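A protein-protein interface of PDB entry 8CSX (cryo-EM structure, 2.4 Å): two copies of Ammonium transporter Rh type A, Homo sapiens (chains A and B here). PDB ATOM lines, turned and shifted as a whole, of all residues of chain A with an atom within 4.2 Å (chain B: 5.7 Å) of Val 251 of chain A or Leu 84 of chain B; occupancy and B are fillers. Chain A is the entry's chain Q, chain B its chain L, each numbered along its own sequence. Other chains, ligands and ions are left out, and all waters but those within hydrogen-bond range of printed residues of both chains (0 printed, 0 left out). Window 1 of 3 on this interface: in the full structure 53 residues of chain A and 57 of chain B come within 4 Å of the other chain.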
ATOM      1  N   LEU A 216      14.012 -13.105 -22.531  1.00  0.00           N
ATOM      2  CA  LEU A 216      12.811 -12.444 -23.006  1.00  0.00           C
ATOM      3  C   LEU A 216      12.986 -10.937 -23.042  1.00  0.00           C
ATOM      4  O   LEU A 216      12.479 -10.282 -23.955  1.00  0.00           O
ATOM      5  CB  LEU A 216      11.613 -12.843 -22.149  1.00  0.00           C
ATOM      6  CG  LEU A 216      11.111 -14.249 -22.459  1.00  0.00           C
ATOM      7  CD1 LEU A 216       9.918 -14.588 -21.612  1.00  0.00           C
ATOM      8  CD2 LEU A 216      10.768 -14.378 -23.932  1.00  0.00           C
ATOM      9  N   TRP A 219      14.939 -10.249 -26.149  1.00  0.00           N
ATOM     10  CA  TRP A 219      14.115 -10.501 -27.324  1.00  0.00           C
ATOM     11  C   TRP A 219      13.116  -9.380 -27.556  1.00  0.00           C
ATOM     12  O   TRP A 219      12.927  -8.935 -28.692  1.00  0.00           O
ATOM     13  CB  TRP A 219      13.393 -11.835 -27.151  1.00  0.00           C
ATOM     14  CG  TRP A 219      12.816 -12.394 -28.386  1.00  0.00           C
ATOM     15  CD1 TRP A 219      13.428 -13.228 -29.265  1.00  0.00           C
ATOM     16  CD2 TRP A 219      11.491 -12.188 -28.882  1.00  0.00           C
ATOM     17  NE1 TRP A 219      12.576 -13.548 -30.285  1.00  0.00           N
ATOM     18  CE2 TRP A 219      11.376 -12.926 -30.073  1.00  0.00           C
ATOM     19  CE3 TRP A 219      10.394 -11.447 -28.438  1.00  0.00           C
ATOM     20  CZ2 TRP A 219      10.211 -12.946 -30.829  1.00  0.00           C
ATOM     21  CZ3 TRP A 219       9.247 -11.464 -29.180  1.00  0.00           C
ATOM     22  CH2 TRP A 219       9.153 -12.218 -30.362  1.00  0.00           C
ATOM     23  N   LEU A 247      13.142 -11.611 -35.443  1.00  0.00           N
ATOM     24  CA  LEU A 247      13.071 -12.338 -34.181  1.00  0.00           C
ATOM     25  C   LEU A 247      11.896 -13.307 -34.159  1.00  0.00           C
ATOM     26  O   LEU A 247      12.023 -14.443 -33.671  1.00  0.00           O
ATOM     27  CB  LEU A 247      12.976 -11.355 -33.019  1.00  0.00           C
ATOM     28  CG  LEU A 247      14.267 -10.608 -32.702  1.00  0.00           C
ATOM     29  CD1 LEU A 247      13.970  -9.361 -31.902  1.00  0.00           C
ATOM     30  CD2 LEU A 247      15.220 -11.510 -31.954  1.00  0.00           C
ATOM     31  N   ALA A 248      10.743 -12.875 -34.682  1.00  0.00           N
ATOM     32  CA  ALA A 248       9.583 -13.762 -34.707  1.00  0.00           C
ATOM     33  C   ALA A 248       9.861 -15.033 -35.509  1.00  0.00           C
ATOM     34  O   ALA A 248       9.496 -16.133 -35.081  1.00  0.00           O
ATOM     35  CB  ALA A 248       8.370 -13.024 -35.266  1.00  0.00           C
ATOM     36  N   ALA A 249      10.509 -14.907 -36.671  1.00  0.00           N
ATOM     37  CA  ALA A 249      10.842 -16.092 -37.468  1.00  0.00           C
ATOM     38  C   ALA A 249      11.928 -16.936 -36.799  1.00  0.00           C
ATOM     39  O   ALA A 249      11.917 -18.182 -36.876  1.00  0.00           O
ATOM     40  CB  ALA A 249      11.279 -15.662 -38.864  1.00  0.00           C
ATOM     41  N   CYS A 250      12.874 -16.265 -36.142  1.00  0.00           N
ATOM     42  CA  CYS A 250      13.972 -16.951 -35.485  1.00  0.00           C
ATOM     43  C   CYS A 250      13.474 -17.872 -34.384  1.00  0.00           C
ATOM     44  O   CYS A 250      14.028 -18.957 -34.184  1.00  0.00           O
ATOM     45  CB  CYS A 250      14.946 -15.919 -34.925  1.00  0.00           C
ATOM     46  SG  CYS A 250      16.411 -16.587 -34.191  1.00  0.00           S
ATOM     47  N   VAL A 251      12.438 -17.451 -33.650  1.00  0.00           N
ATOM     48  CA  VAL A 251      11.902 -18.292 -32.578  1.00  0.00           C
ATOM     49  C   VAL A 251      11.398 -19.621 -33.134  1.00  0.00           C
ATOM     50  O   VAL A 251      11.683 -20.694 -32.584  1.00  0.00           O
ATOM     51  CB  VAL A 251      10.792 -17.551 -31.810  1.00  0.00           C
ATOM     52  CG1 VAL A 251       9.956 -18.533 -30.988  1.00  0.00           C
ATOM     53  CG2 VAL A 251      11.390 -16.508 -30.911  1.00  0.00           C
ATOM     54  N   LEU A 252      10.637 -19.566 -34.229  1.00  0.00           N
ATOM     55  CA  LEU A 252      10.078 -20.782 -34.811  1.00  0.00           C
ATOM     56  C   LEU A 252      11.181 -21.726 -35.263  1.00  0.00           C
ATOM     57  O   LEU A 252      11.141 -22.930 -34.974  1.00  0.00           O
ATOM     58  CB  LEU A 252       9.154 -20.440 -35.983  1.00  0.00           C
ATOM     59  CG  LEU A 252       7.656 -20.246 -35.741  1.00  0.00           C
ATOM     60  CD1 LEU A 252       6.983 -21.566 -35.387  1.00  0.00           C
ATOM     61  CD2 LEU A 252       7.396 -19.190 -34.667  1.00  0.00           C
ATOM     62  N   THR A 253      12.200 -21.192 -35.944  1.00  0.00           N
ATOM     63  CA  THR A 253      13.255 -22.089 -36.416  1.00  0.00           C
ATOM     64  C   THR A 253      14.116 -22.612 -35.268  1.00  0.00           C
ATOM     65  O   THR A 253      14.582 -23.755 -35.313  1.00  0.00           O
ATOM     66  CB  THR A 253      14.121 -21.416 -37.473  1.00  0.00           C
ATOM     67  OG1 THR A 253      14.370 -20.057 -37.107  1.00  0.00           O
ATOM     68  CG2 THR A 253      13.431 -21.484 -38.817  1.00  0.00           C
ATOM     69  N   ALA A 254      14.338 -21.800 -34.232  1.00  0.00           N
ATOM     70  CA  ALA A 254      15.124 -22.255 -33.091  1.00  0.00           C
ATOM     71  C   ALA A 254      14.424 -23.388 -32.353  1.00  0.00           C
ATOM     72  O   ALA A 254      15.052 -24.399 -32.025  1.00  0.00           O
ATOM     73  CB  ALA A 254      15.414 -21.088 -32.150  1.00  0.00           C
ATOM     74  N   PHE A 255      13.116 -23.252 -32.112  1.00  0.00           N
ATOM     75  CA  PHE A 255      12.360 -24.345 -31.501  1.00  0.00           C
ATOM     76  C   PHE A 255      12.387 -25.595 -32.375  1.00  0.00           C
ATOM     77  O   PHE A 255      12.610 -26.708 -31.877  1.00  0.00           O
ATOM     78  CB  PHE A 255      10.912 -23.913 -31.251  1.00  0.00           C
ATOM     79  CG  PHE A 255      10.678 -23.288 -29.905  1.00  0.00           C
ATOM     80  CD1 PHE A 255      10.915 -21.941 -29.698  1.00  0.00           C
ATOM     81  CD2 PHE A 255      10.198 -24.045 -28.850  1.00  0.00           C
ATOM     82  CE1 PHE A 255      10.693 -21.364 -28.466  1.00  0.00           C
ATOM     83  CE2 PHE A 255       9.978 -23.474 -27.618  1.00  0.00           C
ATOM     84  CZ  PHE A 255      10.224 -22.130 -27.427  1.00  0.00           C
ATOM     85  N   THR A 276      17.018 -18.154 -29.891  1.00  0.00           N
ATOM     86  CA  THR A 276      15.882 -17.289 -30.171  1.00  0.00           C
ATOM     87  C   THR A 276      16.273 -15.827 -30.376  1.00  0.00           C
ATOM     88  O   THR A 276      15.430 -15.041 -30.811  1.00  0.00           O
ATOM     89  CB  THR A 276      14.860 -17.405 -29.038  1.00  0.00           C
ATOM     90  OG1 THR A 276      15.504 -17.158 -27.783  1.00  0.00           O
ATOM     91  CG2 THR A 276      14.245 -18.790 -29.015  1.00  0.00           C
ATOM     92  N   PHE B  62       4.995 -11.090 -23.533  1.00  0.00           N
ATOM     93  CA  PHE B  62       6.038 -12.104 -23.423  1.00  0.00           C
ATOM     94  C   PHE B  62       6.504 -12.334 -21.987  1.00  0.00           C
ATOM     95  O   PHE B  62       6.767 -13.472 -21.593  1.00  0.00           O
ATOM     96  CB  PHE B  62       7.195 -11.740 -24.353  1.00  0.00           C
ATOM     97  CG  PHE B  62       6.845 -11.891 -25.799  1.00  0.00           C
ATOM     98  CD1 PHE B  62       7.051 -13.092 -26.445  1.00  0.00           C
ATOM     99  CD2 PHE B  62       6.256 -10.850 -26.497  1.00  0.00           C
ATOM    100  CE1 PHE B  62       6.714 -13.243 -27.763  1.00  0.00           C
ATOM    101  CE2 PHE B  62       5.903 -11.003 -27.817  1.00  0.00           C
ATOM    102  CZ  PHE B  62       6.128 -12.196 -28.451  1.00  0.00           C
ATOM    103  N   SER B  79       5.472 -23.394 -19.895  1.00  0.00           N
ATOM    104  CA  SER B  79       4.682 -22.172 -19.842  1.00  0.00           C
ATOM    105  C   SER B  79       5.423 -21.015 -20.502  1.00  0.00           C
ATOM    106  O   SER B  79       4.936 -20.436 -21.480  1.00  0.00           O
ATOM    107  CB  SER B  79       4.311 -21.842 -18.393  1.00  0.00           C
ATOM    108  OG  SER B  79       5.456 -21.659 -17.596  1.00  0.00           O
ATOM    109  N   VAL B  80       6.652 -20.736 -20.063  1.00  0.00           N
ATOM    110  CA  VAL B  80       7.348 -19.566 -20.593  1.00  0.00           C
ATOM    111  C   VAL B  80       7.785 -19.791 -22.049  1.00  0.00           C
ATOM    112  O   VAL B  80       7.643 -18.899 -22.897  1.00  0.00           O
ATOM    113  CB  VAL B  80       8.507 -19.163 -19.657  1.00  0.00           C
ATOM    114  CG1 VAL B  80       9.685 -20.130 -19.728  1.00  0.00           C
ATOM    115  CG2 VAL B  80       8.939 -17.733 -19.921  1.00  0.00           C
ATOM    116  N   GLY B  81       8.255 -20.998 -22.380  1.00  0.00           N
ATOM    117  CA  GLY B  81       8.769 -21.245 -23.716  1.00  0.00           C
ATOM    118  C   GLY B  81       7.682 -21.350 -24.767  1.00  0.00           C
ATOM    119  O   GLY B  81       7.813 -20.796 -25.860  1.00  0.00           O
ATOM    120  N   ILE B  82       6.604 -22.079 -24.466  1.00  0.00           N
ATOM    121  CA  ILE B  82       5.492 -22.159 -25.400  1.00  0.00           C
ATOM    122  C   ILE B  82       4.785 -20.815 -25.486  1.00  0.00           C
ATOM    123  O   ILE B  82       4.233 -20.466 -26.528  1.00  0.00           O
ATOM    124  CB  ILE B  82       4.530 -23.301 -25.010  1.00  0.00           C
ATOM    125  CG1 ILE B  82       5.280 -24.636 -24.924  1.00  0.00           C
ATOM    126  CG2 ILE B  82       3.408 -23.435 -26.017  1.00  0.00           C
ATOM    127  CD1 ILE B  82       6.143 -24.943 -26.121  1.00  0.00           C
ATOM    128  N   ASN B  83       4.819 -20.020 -24.411  1.00  0.00           N
ATOM    129  CA  ASN B  83       4.351 -18.647 -24.523  1.00  0.00           C
ATOM    130  C   ASN B  83       5.150 -17.888 -25.576  1.00  0.00           C
ATOM    131  O   ASN B  83       4.569 -17.254 -26.465  1.00  0.00           O
ATOM    132  CB  ASN B  83       4.446 -17.959 -23.163  1.00  0.00           C
ATOM    133  CG  ASN B  83       3.640 -16.685 -23.096  1.00  0.00           C
ATOM    134  OD1 ASN B  83       2.468 -16.706 -22.732  1.00  0.00           O
ATOM    135  ND2 ASN B  83       4.269 -15.564 -23.420  1.00  0.00           N
ATOM    136  N   LEU B  84       6.483 -17.983 -25.515  1.00  0.00           N
ATOM    137  CA  LEU B  84       7.320 -17.330 -26.520  1.00  0.00           C
ATOM    138  C   LEU B  84       7.023 -17.852 -27.925  1.00  0.00           C
ATOM    139  O   LEU B  84       6.862 -17.068 -28.864  1.00  0.00           O
ATOM    140  CB  LEU B  84       8.801 -17.520 -26.180  1.00  0.00           C
ATOM    141  CG  LEU B  84       9.854 -17.006 -27.170  1.00  0.00           C
ATOM    142  CD1 LEU B  84       9.683 -15.524 -27.469  1.00  0.00           C
ATOM    143  CD2 LEU B  84      11.247 -17.278 -26.644  1.00  0.00           C
ATOM    144  N   LEU B  85       6.909 -19.174 -28.072  1.00  0.00           N
ATOM    145  CA  LEU B  85       6.717 -19.786 -29.383  1.00  0.00           C
ATOM    146  C   LEU B  85       5.359 -19.425 -29.979  1.00  0.00           C
ATOM    147  O   LEU B  85       5.263 -19.023 -31.146  1.00  0.00           O
ATOM    148  CB  LEU B  85       6.869 -21.303 -29.257  1.00  0.00           C
ATOM    149  CG  LEU B  85       6.454 -22.199 -30.423  1.00  0.00           C
ATOM    150  CD1 LEU B  85       7.466 -22.148 -31.550  1.00  0.00           C
ATOM    151  CD2 LEU B  85       6.245 -23.624 -29.947  1.00  0.00           C
ATOM    152  N   VAL B  86       4.301 -19.559 -29.179  1.00  0.00           N
ATOM    153  CA  VAL B  86       2.949 -19.249 -29.611  1.00  0.00           C
ATOM    154  C   VAL B  86       2.829 -17.781 -29.974  1.00  0.00           C
ATOM    155  O   VAL B  86       2.246 -17.439 -31.002  1.00  0.00           O
ATOM    156  CB  VAL B  86       1.944 -19.654 -28.515  1.00  0.00           C
ATOM    157  CG1 VAL B  86       0.656 -18.878 -28.648  1.00  0.00           C
ATOM    158  CG2 VAL B  86       1.666 -21.145 -28.575  1.00  0.00           C
ATOM    159  N   ALA B  87       3.399 -16.890 -29.162  1.00  0.00           N
ATOM    160  CA  ALA B  87       3.275 -15.470 -29.462  1.00  0.00           C
ATOM    161  C   ALA B  87       4.106 -15.076 -30.681  1.00  0.00           C
ATOM    162  O   ALA B  87       3.693 -14.208 -31.457  1.00  0.00           O
ATOM    163  CB  ALA B  87       3.660 -14.651 -28.237  1.00  0.00           C
ATOM    164  N   ALA B  88       5.265 -15.710 -30.882  1.00  0.00           N
ATOM    165  CA  ALA B  88       6.075 -15.408 -32.059  1.00  0.00           C
ATOM    166  C   ALA B  88       5.389 -15.854 -33.342  1.00  0.00           C
ATOM    167  O   ALA B  88       5.405 -15.131 -34.344  1.00  0.00           O
ATOM    168  CB  ALA B  88       7.450 -16.058 -31.939  1.00  0.00           C
ATOM    169  N   LEU B  89       4.799 -17.050 -33.340  1.00  0.00           N
ATOM    170  CA  LEU B  89       4.000 -17.460 -34.489  1.00  0.00           C
ATOM    171  C   LEU B  89       2.776 -16.567 -34.640  1.00  0.00           C
ATOM    172  O   LEU B  89       2.398 -16.190 -35.761  1.00  0.00           O
ATOM    173  CB  LEU B  89       3.589 -18.927 -34.350  1.00  0.00           C
ATOM    174  CG  LEU B  89       2.575 -19.439 -35.376  1.00  0.00           C
ATOM    175  CD1 LEU B  89       3.156 -19.413 -36.778  1.00  0.00           C
ATOM    176  CD2 LEU B  89       2.067 -20.827 -35.028  1.00  0.00           C
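Printed residues of chain B that touch a printed residue of chain A: Phe 62, Val 80, Gly 81, Leu 84, Leu 85, Ala 88 and Leu 89. Hydrophobic or aromatic side chains of chain B that line the printed part of chain A: Phe 62, Val 80, Leu 84, Leu 85, Ala 88 and Leu 89. Along chain B the printed residues that touch a printed residue of chain A span positions 62 to 89. Of the 12 printed residues of chain A, 6 touch a printed residue of chain B.
No position is printed for both chains. Of the 12 pairs that touch across the chains among the printed residues, none has its exchanged pair printed and touching as well.
Among the printed residues, pairs that only touch across the chains: Phe 255 of chain A with Gly 81 of chain B (3.2 Å), Trp 219 of chain A with Phe 62 of chain B (3.3 Å), Leu 216 of chain A with Phe 62 of chain B (3.3 Å), Leu 252 of chain A with Leu 89 of chain B (3.6 Å), Val 251 of chain A with Ala 88 of chain B (3.6 Å), Leu 216 of chain A with Val 80 of chain B (3.7 Å), Ala 248 of chain A with Ala 88 of chain B (3.8 Å), Phe 255 of chain A with Leu 85 of chain B (3.8 Å), Val 251 of chain A with Leu 85 of chain B (3.8 Å), Leu 216 of chain A with Leu 84 of chain B (3.9 Å), Leu 252 of chain A with Leu 85 of chain B (3.9 Å) and Val 251 of chain A with Leu 84 of chain B (3.97 Å).
Val 251 of chain A touches just these residues of chain B: Leu 84 (3.97 Å), Leu 85 (3.8 Å) and Ala 88 (3.6 Å). Of the printed residues of chain A, Phe 62 of chain B touches Leu 216 and Trp 219. Of the printed residues of chain A, Gly 81 of chain B touches Phe 255 (3.2 Å). Printed residues of chain A within 4 Å of Leu 84 of chain B: Leu 216 (3.9 Å) and Val 251 (3.97 Å). Of the printed residues of chain A, Leu 85 of chain B touches Val 251, Leu 252 and Phe 255. Of the printed residues of chain A, Ala 88 of chain B touches Ala 248 (3.8 Å) and Val 251 (3.6 Å). The nearest printed residue of chain B that does not touch Trp 219 of chain A is Leu 84 of chain B (4.05 Å).
NE1 of Trp 219 of chain A sits close to O of Thr 276 of chain A.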
